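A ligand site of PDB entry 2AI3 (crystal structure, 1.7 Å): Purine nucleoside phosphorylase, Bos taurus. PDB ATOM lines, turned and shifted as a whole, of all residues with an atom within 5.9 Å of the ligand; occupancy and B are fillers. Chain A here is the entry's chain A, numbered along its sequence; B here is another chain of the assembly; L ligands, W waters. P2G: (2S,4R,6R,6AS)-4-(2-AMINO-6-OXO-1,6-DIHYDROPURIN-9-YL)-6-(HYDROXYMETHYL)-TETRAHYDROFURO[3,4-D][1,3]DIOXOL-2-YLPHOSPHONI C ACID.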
ATOM      1  N   GLY A  32      20.649   9.266   4.559  1.00  0.00           N
ATOM      2  CA  GLY A  32      19.259   9.535   4.896  1.00  0.00           C
ATOM      3  C   GLY A  32      18.220   8.671   4.200  1.00  0.00           C
ATOM      4  O   GLY A  32      18.550   7.640   3.620  1.00  0.00           O
ATOM      5  N   SER A  33      16.961   9.104   4.265  1.00  0.00           N
ATOM      6  CA  SER A  33      15.855   8.376   3.651  1.00  0.00           C
ATOM      7  C   SER A  33      16.036   8.145   2.146  1.00  0.00           C
ATOM      8  O   SER A  33      16.147   9.103   1.379  1.00  0.00           O
ATOM      9  CB  SER A  33      14.528   9.118   3.884  1.00  0.00           C
ATOM     10  OG  SER A  33      14.158   9.090   5.257  1.00  0.00           O
ATOM     11  N   LEU A  35      18.552   7.057   0.659  1.00  0.00           N
ATOM     12  CA  LEU A  35      19.905   7.384   0.226  1.00  0.00           C
ATOM     13  C   LEU A  35      20.899   6.315   0.659  1.00  0.00           C
ATOM     14  O   LEU A  35      22.112   6.508   0.604  1.00  0.00           O
ATOM     15  CB  LEU A  35      20.321   8.738   0.815  1.00  0.00           C
ATOM     16  CG  LEU A  35      19.340   9.897   0.608  1.00  0.00           C
ATOM     17  CD1 LEU A  35      19.895  11.163   1.242  1.00  0.00           C
ATOM     18  CD2 LEU A  35      19.095  10.113  -0.895  1.00  0.00           C
ATOM     19  N   ARG A  84      19.227   6.157   9.843  1.00  0.00           N
ATOM     20  CA  ARG A  84      19.554   6.982  11.003  1.00  0.00           C
ATOM     21  C   ARG A  84      18.429   6.947  12.035  1.00  0.00           C
ATOM     22  O   ARG A  84      17.468   6.187  11.875  1.00  0.00           O
ATOM     23  CB  ARG A  84      19.850   8.437  10.589  1.00  0.00           C
ATOM     24  CG  ARG A  84      18.735   9.111   9.792  1.00  0.00           C
ATOM     25  CD  ARG A  84      18.612  10.598  10.165  1.00  0.00           C
ATOM     26  NE  ARG A  84      19.829  11.382   9.908  1.00  0.00           N
ATOM     27  CZ  ARG A  84      20.200  11.855   8.729  1.00  0.00           C
ATOM     28  NH1 ARG A  84      19.456  11.642   7.638  1.00  0.00           N
ATOM     29  NH2 ARG A  84      21.309  12.581   8.626  1.00  0.00           N
ATOM     30  N   HIS A  86      15.593   9.195  14.556  1.00  0.00           N
ATOM     31  CA  HIS A  86      14.865  10.466  14.572  1.00  0.00           C
ATOM     32  C   HIS A  86      14.165  10.777  15.887  1.00  0.00           C
ATOM     33  O   HIS A  86      13.697   9.881  16.596  1.00  0.00           O
ATOM     34  CB  HIS A  86      13.795  10.490  13.472  1.00  0.00           C
ATOM     35  CG  HIS A  86      14.321  10.232  12.091  1.00  0.00           C
ATOM     36  ND1 HIS A  86      14.598   8.967  11.627  1.00  0.00           N
ATOM     37  CD2 HIS A  86      14.626  11.086  11.083  1.00  0.00           C
ATOM     38  CE1 HIS A  86      15.046   9.049  10.380  1.00  0.00           C
ATOM     39  NE2 HIS A  86      15.070  10.318  10.030  1.00  0.00           N
ATOM     40  N   TYR A  88      11.275  12.026  16.294  1.00  0.00           N
ATOM     41  CA  TYR A  88       9.869  11.615  16.263  1.00  0.00           C
ATOM     42  C   TYR A  88       9.625  10.147  16.614  1.00  0.00           C
ATOM     43  O   TYR A  88       8.487   9.738  16.837  1.00  0.00           O
ATOM     44  CB  TYR A  88       9.224  11.935  14.906  1.00  0.00           C
ATOM     45  CG  TYR A  88       9.825  11.226  13.714  1.00  0.00           C
ATOM     46  CD1 TYR A  88       9.679   9.849  13.543  1.00  0.00           C
ATOM     47  CD2 TYR A  88      10.524  11.943  12.735  1.00  0.00           C
ATOM     48  CE1 TYR A  88      10.233   9.199  12.432  1.00  0.00           C
ATOM     49  CE2 TYR A  88      11.074  11.307  11.632  1.00  0.00           C
ATOM     50  CZ  TYR A  88      10.931   9.940  11.491  1.00  0.00           C
ATOM     51  OH  TYR A  88      11.478   9.320  10.397  1.00  0.00           O
ATOM     52  N   THR A 114      23.742  13.545   5.012  1.00  0.00           N
ATOM     53  CA  THR A 114      22.823  13.719   3.887  1.00  0.00           C
ATOM     54  C   THR A 114      21.392  13.486   4.363  1.00  0.00           C
ATOM     55  O   THR A 114      21.165  12.823   5.364  1.00  0.00           O
ATOM     56  CB  THR A 114      23.121  12.711   2.756  1.00  0.00           C
ATOM     57  OG1 THR A 114      22.687  11.407   3.151  1.00  0.00           O
ATOM     58  CG2 THR A 114      24.607  12.669   2.451  1.00  0.00           C
ATOM     59  N   ASN A 115      20.425  14.053   3.633  1.00  0.00           N
ATOM     60  CA  ASN A 115      19.021  13.875   3.977  1.00  0.00           C
ATOM     61  C   ASN A 115      18.116  14.212   2.809  1.00  0.00           C
ATOM     62  O   ASN A 115      18.565  14.690   1.770  1.00  0.00           O
ATOM     63  CB  ASN A 115      18.631  14.728   5.201  1.00  0.00           C
ATOM     64  CG  ASN A 115      18.722  16.232   4.941  1.00  0.00           C
ATOM     65  OD1 ASN A 115      18.210  16.740   3.946  1.00  0.00           O
ATOM     66  ND2 ASN A 115      19.357  16.957   5.863  1.00  0.00           N
ATOM     67  N   ALA A 116      16.826  13.926   2.984  1.00  0.00           N
ATOM     68  CA  ALA A 116      15.814  14.230   1.998  1.00  0.00           C
ATOM     69  C   ALA A 116      15.028  15.382   2.614  1.00  0.00           C
ATOM     70  O   ALA A 116      14.720  15.359   3.802  1.00  0.00           O
ATOM     71  CB  ALA A 116      14.895  13.018   1.791  1.00  0.00           C
ATOM     72  N   ALA A 117      14.729  16.404   1.813  1.00  0.00           N
ATOM     73  CA  ALA A 117      14.009  17.558   2.345  1.00  0.00           C
ATOM     74  C   ALA A 117      12.991  18.187   1.391  1.00  0.00           C
ATOM     75  O   ALA A 117      13.025  17.965   0.181  1.00  0.00           O
ATOM     76  CB  ALA A 117      15.008  18.612   2.787  1.00  0.00           C
ATOM     77  N   GLY A 118      12.095  18.975   1.975  1.00  0.00           N
ATOM     78  CA  GLY A 118      11.083  19.674   1.198  1.00  0.00           C
ATOM     79  C   GLY A 118      11.652  21.028   0.805  1.00  0.00           C
ATOM     80  O   GLY A 118      12.269  21.705   1.628  1.00  0.00           O
ATOM     81  N   GLY A 119      11.430  21.425  -0.439  1.00  0.00           N
ATOM     82  CA  GLY A 119      11.946  22.707  -0.902  1.00  0.00           C
ATOM     83  C   GLY A 119      11.083  23.903  -0.583  1.00  0.00           C
ATOM     84  O   GLY A 119       9.920  23.970  -1.000  1.00  0.00           O
ATOM     85  N   TYR A 192      19.111  24.926   5.964  1.00  0.00           N
ATOM     86  CA  TYR A 192      18.241  23.803   6.322  1.00  0.00           C
ATOM     87  C   TYR A 192      17.626  24.052   7.682  1.00  0.00           C
ATOM     88  O   TYR A 192      18.325  24.409   8.634  1.00  0.00           O
ATOM     89  CB  TYR A 192      19.067  22.510   6.370  1.00  0.00           C
ATOM     90  CG  TYR A 192      18.299  21.275   6.820  1.00  0.00           C
ATOM     91  CD1 TYR A 192      17.629  20.464   5.890  1.00  0.00           C
ATOM     92  CD2 TYR A 192      18.256  20.898   8.161  1.00  0.00           C
ATOM     93  CE1 TYR A 192      16.954  19.311   6.294  1.00  0.00           C
ATOM     94  CE2 TYR A 192      17.571  19.752   8.583  1.00  0.00           C
ATOM     95  CZ  TYR A 192      16.934  18.966   7.635  1.00  0.00           C
ATOM     96  OH  TYR A 192      16.288  17.816   8.032  1.00  0.00           O
ATOM     97  N   LEU A 195      12.606  20.456  12.106  1.00  0.00           N
ATOM     98  CA  LEU A 195      11.454  20.453  13.000  1.00  0.00           C
ATOM     99  C   LEU A 195      11.245  18.998  13.414  1.00  0.00           C
ATOM    100  O   LEU A 195      11.739  18.069  12.755  1.00  0.00           O
ATOM    101  CB  LEU A 195      10.201  21.056  12.334  1.00  0.00           C
ATOM    102  CG  LEU A 195       9.834  20.791  10.888  1.00  0.00           C
ATOM    103  CD1 LEU A 195       9.473  19.335  10.688  1.00  0.00           C
ATOM    104  CD2 LEU A 195       8.659  21.695  10.519  1.00  0.00           C
ATOM    105  N   ASN A 199       4.357  14.412  11.576  1.00  0.00           N
ATOM    106  CA  ASN A 199       3.390  14.881  10.591  1.00  0.00           C
ATOM    107  C   ASN A 199       4.036  15.895   9.651  1.00  0.00           C
ATOM    108  O   ASN A 199       5.042  16.524   9.999  1.00  0.00           O
ATOM    109  CB  ASN A 199       2.176  15.529  11.260  1.00  0.00           C
ATOM    110  CG  ASN A 199       2.532  16.803  12.001  1.00  0.00           C
ATOM    111  OD1 ASN A 199       2.957  16.766  13.157  1.00  0.00           O
ATOM    112  ND2 ASN A 199       2.365  17.938  11.338  1.00  0.00           N
ATOM    113  N   PHE A 200       3.471  16.059   8.458  1.00  0.00           N
ATOM    114  CA  PHE A 200       3.992  17.040   7.525  1.00  0.00           C
ATOM    115  C   PHE A 200       3.377  18.403   7.840  1.00  0.00           C
ATOM    116  O   PHE A 200       2.326  18.475   8.477  1.00  0.00           O
ATOM    117  CB  PHE A 200       3.681  16.611   6.080  1.00  0.00           C
ATOM    118  CG  PHE A 200       4.562  15.501   5.593  1.00  0.00           C
ATOM    119  CD1 PHE A 200       5.941  15.685   5.479  1.00  0.00           C
ATOM    120  CD2 PHE A 200       4.022  14.261   5.252  1.00  0.00           C
ATOM    121  CE1 PHE A 200       6.768  14.651   5.040  1.00  0.00           C
ATOM    122  CE2 PHE A 200       4.843  13.219   4.813  1.00  0.00           C
ATOM    123  CZ  PHE A 200       6.219  13.418   4.707  1.00  0.00           C
ATOM    124  N   GLU A 201       4.035  19.470   7.391  1.00  0.00           N
ATOM    125  CA  GLU A 201       3.601  20.836   7.677  1.00  0.00           C
ATOM    126  C   GLU A 201       2.321  21.347   7.005  1.00  0.00           C
ATOM    127  O   GLU A 201       1.946  20.890   5.928  1.00  0.00           O
ATOM    128  CB  GLU A 201       4.722  21.826   7.330  1.00  0.00           C
ATOM    129  CG  GLU A 201       6.059  21.608   8.044  1.00  0.00           C
ATOM    130  CD  GLU A 201       6.786  20.362   7.581  1.00  0.00           C
ATOM    131  OE1 GLU A 201       6.790  20.063   6.364  1.00  0.00           O
ATOM    132  OE2 GLU A 201       7.384  19.680   8.439  1.00  0.00           O
ATOM    133  N   VAL A 217      13.344  22.073   4.342  1.00  0.00           N
ATOM    134  CA  VAL A 217      12.876  21.621   5.660  1.00  0.00           C
ATOM    135  C   VAL A 217      12.878  20.099   5.812  1.00  0.00           C
ATOM    136  O   VAL A 217      12.458  19.366   4.915  1.00  0.00           O
ATOM    137  CB  VAL A 217      11.447  22.166   5.938  1.00  0.00           C
ATOM    138  CG1 VAL A 217      10.503  21.777   4.828  1.00  0.00           C
ATOM    139  CG2 VAL A 217      10.922  21.645   7.285  1.00  0.00           C
ATOM    140  N   GLY A 218      13.344  19.636   6.968  1.00  0.00           N
ATOM    141  CA  GLY A 218      13.391  18.205   7.239  1.00  0.00           C
ATOM    142  C   GLY A 218      13.246  17.877   8.716  1.00  0.00           C
ATOM    143  O   GLY A 218      13.022  18.769   9.532  1.00  0.00           O
ATOM    144  N   MET A 219      13.397  16.592   9.067  1.00  0.00           N
ATOM    145  CA  MET A 219      13.251  16.155  10.462  1.00  0.00           C
ATOM    146  C   MET A 219      14.516  15.543  11.090  1.00  0.00           C
ATOM    147  O   MET A 219      14.422  14.758  12.046  1.00  0.00           O
ATOM    148  CB  MET A 219      12.110  15.142  10.555  1.00  0.00           C
ATOM    149  CG  MET A 219      10.824  15.570   9.850  1.00  0.00           C
ATOM    150  SD  MET A 219       9.537  14.281   9.848  1.00  0.00           S
ATOM    151  CE  MET A 219       8.200  15.117   9.001  1.00  0.00           C
ATOM    152  N   SER A 220      15.705  15.902  10.594  1.00  0.00           N
ATOM    153  CA  SER A 220      16.933  15.319  11.134  1.00  0.00           C
ATOM    154  C   SER A 220      18.146  16.217  10.938  1.00  0.00           C
ATOM    155  O   SER A 220      18.029  17.440  10.839  1.00  0.00           O
ATOM    156  CB  SER A 220      17.204  13.984  10.422  1.00  0.00           C
ATOM    157  OG  SER A 220      17.589  14.211   9.074  1.00  0.00           O
ATOM    158  N   THR A 221      19.308  15.569  10.960  1.00  0.00           N
ATOM    159  CA  THR A 221      20.611  16.192  10.687  1.00  0.00           C
ATOM    160  C   THR A 221      21.206  17.219  11.660  1.00  0.00           C
ATOM    161  O   THR A 221      22.352  17.078  12.081  1.00  0.00           O
ATOM    162  CB  THR A 221      20.563  16.784   9.266  1.00  0.00           C
ATOM    163  OG1 THR A 221      20.142  15.755   8.355  1.00  0.00           O
ATOM    164  CG2 THR A 221      21.929  17.299   8.828  1.00  0.00           C
ATOM    165  N   THR A 242      13.278  16.458  -2.569  1.00  0.00           N
ATOM    166  CA  THR A 242      12.358  15.458  -3.088  1.00  0.00           C
ATOM    167  C   THR A 242      11.010  16.006  -3.518  1.00  0.00           C
ATOM    168  O   THR A 242      10.244  15.314  -4.206  1.00  0.00           O
ATOM    169  CB  THR A 242      12.123  14.330  -2.048  1.00  0.00           C
ATOM    170  OG1 THR A 242      11.588  14.892  -0.846  1.00  0.00           O
ATOM    171  CG2 THR A 242      13.435  13.636  -1.731  1.00  0.00           C
ATOM    172  N   ASN A 243      10.697  17.235  -3.136  1.00  0.00           N
ATOM    173  CA  ASN A 243       9.421  17.830  -3.500  1.00  0.00           C
ATOM    174  C   ASN A 243       9.352  19.326  -3.183  1.00  0.00           C
ATOM    175  O   ASN A 243      10.036  19.805  -2.284  1.00  0.00           O
ATOM    176  CB  ASN A 243       8.288  17.107  -2.774  1.00  0.00           C
ATOM    177  CG  ASN A 243       8.298  17.360  -1.269  1.00  0.00           C
ATOM    178  OD1 ASN A 243       7.796  18.368  -0.799  1.00  0.00           O
ATOM    179  ND2 ASN A 243       8.890  16.435  -0.522  1.00  0.00           N
ATOM    180  N   VAL A 245       7.316  22.204  -1.642  1.00  0.00           N
ATOM    181  CA  VAL A 245       6.209  22.391  -0.719  1.00  0.00           C
ATOM    182  C   VAL A 245       5.227  23.439  -1.229  1.00  0.00           C
ATOM    183  O   VAL A 245       5.638  24.475  -1.755  1.00  0.00           O
ATOM    184  CB  VAL A 245       6.711  22.817   0.699  1.00  0.00           C
ATOM    185  CG1 VAL A 245       7.758  21.820   1.193  1.00  0.00           C
ATOM    186  CG2 VAL A 245       7.278  24.222   0.655  1.00  0.00           C
ATOM    187  N   ALA A 255       1.683  15.617   0.440  1.00  0.00           N
ATOM    188  CA  ALA A 255       2.993  14.986   0.610  1.00  0.00           C
ATOM    189  C   ALA A 255       2.880  13.658   1.348  1.00  0.00           C
ATOM    190  O   ALA A 255       2.166  13.547   2.354  1.00  0.00           O
ATOM    191  CB  ALA A 255       3.927  15.926   1.367  1.00  0.00           C
ATOM    192  N   ASN A 256       3.574  12.646   0.840  1.00  0.00           N
ATOM    193  CA  ASN A 256       3.567  11.328   1.449  1.00  0.00           C
ATOM    194  C   ASN A 256       4.988  10.790   1.583  1.00  0.00           C
ATOM    195  O   ASN A 256       5.952  11.473   1.215  1.00  0.00           O
ATOM    196  CB  ASN A 256       2.718  10.364   0.612  1.00  0.00           C
ATOM    197  CG  ASN A 256       3.171  10.282  -0.833  1.00  0.00           C
ATOM    198  OD1 ASN A 256       4.286   9.817  -1.125  1.00  0.00           O
ATOM    199  ND2 ASN A 256       2.329  10.733  -1.750  1.00  0.00           N
ATOM    200  N   HIS A 257       5.125   9.577   2.099  1.00  0.00           N
ATOM    201  CA  HIS A 257       6.443   8.965   2.298  1.00  0.00           C
ATOM    202  C   HIS A 257       7.007   8.308   1.037  1.00  0.00           C
ATOM    203  O   HIS A 257       8.209   8.324   0.815  1.00  0.00           O
ATOM    204  CB  HIS A 257       6.382   7.946   3.440  1.00  0.00           C
ATOM    205  CG  HIS A 257       7.708   7.364   3.790  1.00  0.00           C
ATOM    206  ND1 HIS A 257       8.782   8.128   4.165  1.00  0.00           N
ATOM    207  CD2 HIS A 257       8.138   6.074   3.821  1.00  0.00           C
ATOM    208  CE1 HIS A 257       9.820   7.349   4.416  1.00  0.00           C
ATOM    209  NE2 HIS A 257       9.455   6.094   4.218  1.00  0.00           N
ATOM    210  N   VAL A 260       9.058  10.649  -1.357  1.00  0.00           N
ATOM    211  CA  VAL A 260      10.467  10.885  -1.018  1.00  0.00           C
ATOM    212  C   VAL A 260      11.255   9.608  -1.248  1.00  0.00           C
ATOM    213  O   VAL A 260      12.460   9.646  -1.533  1.00  0.00           O
ATOM    214  CB  VAL A 260      10.626  11.301   0.461  1.00  0.00           C
ATOM    215  CG1 VAL A 260      12.091  11.460   0.804  1.00  0.00           C
ATOM    216  CG2 VAL A 260       9.869  12.594   0.725  1.00  0.00           C
ATOM    217  N   PHE B 159       3.668   9.078   8.801  1.00  0.00           N
ATOM    218  CA  PHE B 159       3.832  10.479   8.417  1.00  0.00           C
ATOM    219  C   PHE B 159       2.548  11.080   7.848  1.00  0.00           C
ATOM    220  O   PHE B 159       2.421  11.271   6.634  1.00  0.00           O
ATOM    221  CB  PHE B 159       4.947  10.596   7.357  1.00  0.00           C
ATOM    222  CG  PHE B 159       6.252  10.005   7.785  1.00  0.00           C
ATOM    223  CD1 PHE B 159       7.049  10.650   8.734  1.00  0.00           C
ATOM    224  CD2 PHE B 159       6.706   8.810   7.245  1.00  0.00           C
ATOM    225  CE1 PHE B 159       8.270  10.108   9.128  1.00  0.00           C
ATOM    226  CE2 PHE B 159       7.936   8.261   7.631  1.00  0.00           C
ATOM    227  CZ  PHE B 159       8.718   8.916   8.567  1.00  0.00           C
HETATM  228  O6  P2G L   1       8.038  18.933   3.224  1.00  0.00           O
HETATM  229  C6  P2G L   1       8.722  18.238   3.972  1.00  0.00           C
HETATM  230  N1  P2G L   1       8.696  18.516   5.360  1.00  0.00           N
HETATM  231  C2  P2G L   1       9.421  17.729   6.272  1.00  0.00           C
HETATM  232  N2  P2G L   1       9.490  18.074   7.544  1.00  0.00           N
HETATM  233  N3  P2G L   1      10.120  16.689   5.758  1.00  0.00           N
HETATM  234  C4  P2G L   1      10.161  16.400   4.443  1.00  0.00           C
HETATM  235  C5  P2G L   1       9.472  17.173   3.486  1.00  0.00           C
HETATM  236  N7  P2G L   1       9.765  16.675   2.290  1.00  0.00           N
HETATM  237  C8  P2G L   1      10.591  15.654   2.467  1.00  0.00           C
HETATM  238  N9  P2G L   1      10.825  15.459   3.765  1.00  0.00           N
HETATM  239  C1' P2G L   1      11.387  14.172   4.256  1.00  0.00           C
HETATM  240  O4' P2G L   1      10.245  13.334   4.506  1.00  0.00           O
HETATM  241  C2' P2G L   1      12.233  14.125   5.533  1.00  0.00           C
HETATM  242  O2' P2G L   1      13.603  13.711   5.348  1.00  0.00           O
HETATM  243  C1  P2G L   1      13.783  12.405   5.937  1.00  0.00           C
HETATM  244  P   P2G L   1      15.474  12.189   6.632  1.00  0.00           P
HETATM  245  O3  P2G L   1      15.569  10.883   7.554  1.00  0.00           O
HETATM  246  O4  P2G L   1      15.683  13.483   7.566  1.00  0.00           O
HETATM  247  O2  P2G L   1      16.466  12.110   5.534  1.00  0.00           O
HETATM  248  O3' P2G L   1      12.726  12.345   6.908  1.00  0.00           O
HETATM  249  C3' P2G L   1      11.578  13.044   6.388  1.00  0.00           C
HETATM  250  C4' P2G L   1      10.705  12.294   5.378  1.00  0.00           C
HETATM  251  C5' P2G L   1       9.526  11.556   6.019  1.00  0.00           C
HETATM  252  O5' P2G L   1       8.696  11.047   4.974  1.00  0.00           O
HETATM  253  O   HOH W   1      15.555  15.802   6.410  1.00  0.00           O
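ND2 of Asn 243 is in hydrogen-bond range of N7 of the ligand. The backbone NH (N) of Gly 118 sits at hydrogen-bond distance from a nitrogen (N7) of the ligand, 3.3 Å away. The backbone NH (N) of Ser 33 lies within hydrogen-bond range of an oxygen (O2) of the ligand (3.3 Å). N of Ala 116 lies within hydrogen-bond range of O2 of the ligand (3.2 Å). A ring nitrogen (NE2) of His 86 lies within hydrogen-bond range of an oxygen (O3) of the ligand (2.6 Å). O5' of the ligand lies within hydrogen-bond range of ND1 of His 257, 3.0 Å away. The side-chain hydroxyl (OG) of Ser 220 sits at hydrogen-bond distance from an oxygen (O4) of the ligand. A nitrogen (N1) of the ligand lies within hydrogen-bond range of the side-chain carboxylate (OE1) of Glu 201 (2.7 Å). An oxygen (O2') of the ligand sits close to the backbone carbonyl oxygen (O) of Ala 116, at 2.5 Å. An oxygen (O3) of the ligand sits at hydrogen-bond distance from the side-chain hydroxyl (OG) of Ser 33 (3.2 Å). NH1 of Arg 84 is in salt-bridge range of O2 of the ligand.
NH1 of Arg 84 is in hydrogen-bond range of O of Thr 114, 3.1 Å away. The backbone NH of Leu 195 sits at hydrogen-bond distance from the backbone carbonyl oxygen of Gly 218, at 3.1 Å. The backbone carbonyl oxygen (O) of Gly 118 lies within hydrogen-bond range of the backbone NH (N) of Val 217. The backbone NH of Gly 32 lies within hydrogen-bond range of the side-chain hydroxyl of Thr 114 (3.3 Å). ND1 of His 86 is in hydrogen-bond range of OH of Tyr 88 (3.4 Å). N of Ser 220 is in hydrogen-bond range of OH of Tyr 192 (3.3 Å). The side-chain amide nitrogen of Asn 243 sits at hydrogen-bond distance from the side-chain hydroxyl of Thr 242. The backbone NH (N) of Thr 242 sits at hydrogen-bond distance from the backbone carbonyl oxygen (O) of Ala 117 (3.1 Å).
Merely in contact with the ligand: Gly 32 (3.9 Å), Asn 115 (3.4 Å), Ala 117 (3.7 Å), Leu 195 (3.4 Å), Phe 200 (3.4 Å), Val 217 (3.7 Å), Gly 218 (3.9 Å), Met 219 (3.5 Å), Thr 242 (3.5 Å), Val 245 (3.5 Å), Val 260 (3.6 Å) and Phe 159 of chain B (3.7 Å). Hydrophobic or aromatic side chains that line the ligand: His 86, Ala 116, Leu 195, Phe 200, Val 217, Met 219, Val 245, His 257, Val 260 and Phe 159 of chain B. 21 residues have an atom within 4 Å of the ligand: Gly 32, Ser 33, Arg 84, His 86, Asn 115, Ala 116, Ala 117, Gly 118, Leu 195, Phe 200, Glu 201, Val 217, Gly 218, Met 219, Ser 220, Thr 242, Asn 243, Val 245, His 257, Val 260 and Phe 159 of chain B.
Water W1 lies within hydrogen-bond range of an oxygen (O4) of the ligand, the side-chain hydroxyl of Tyr 192 and the backbone carbonyl oxygen of Ala 116.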
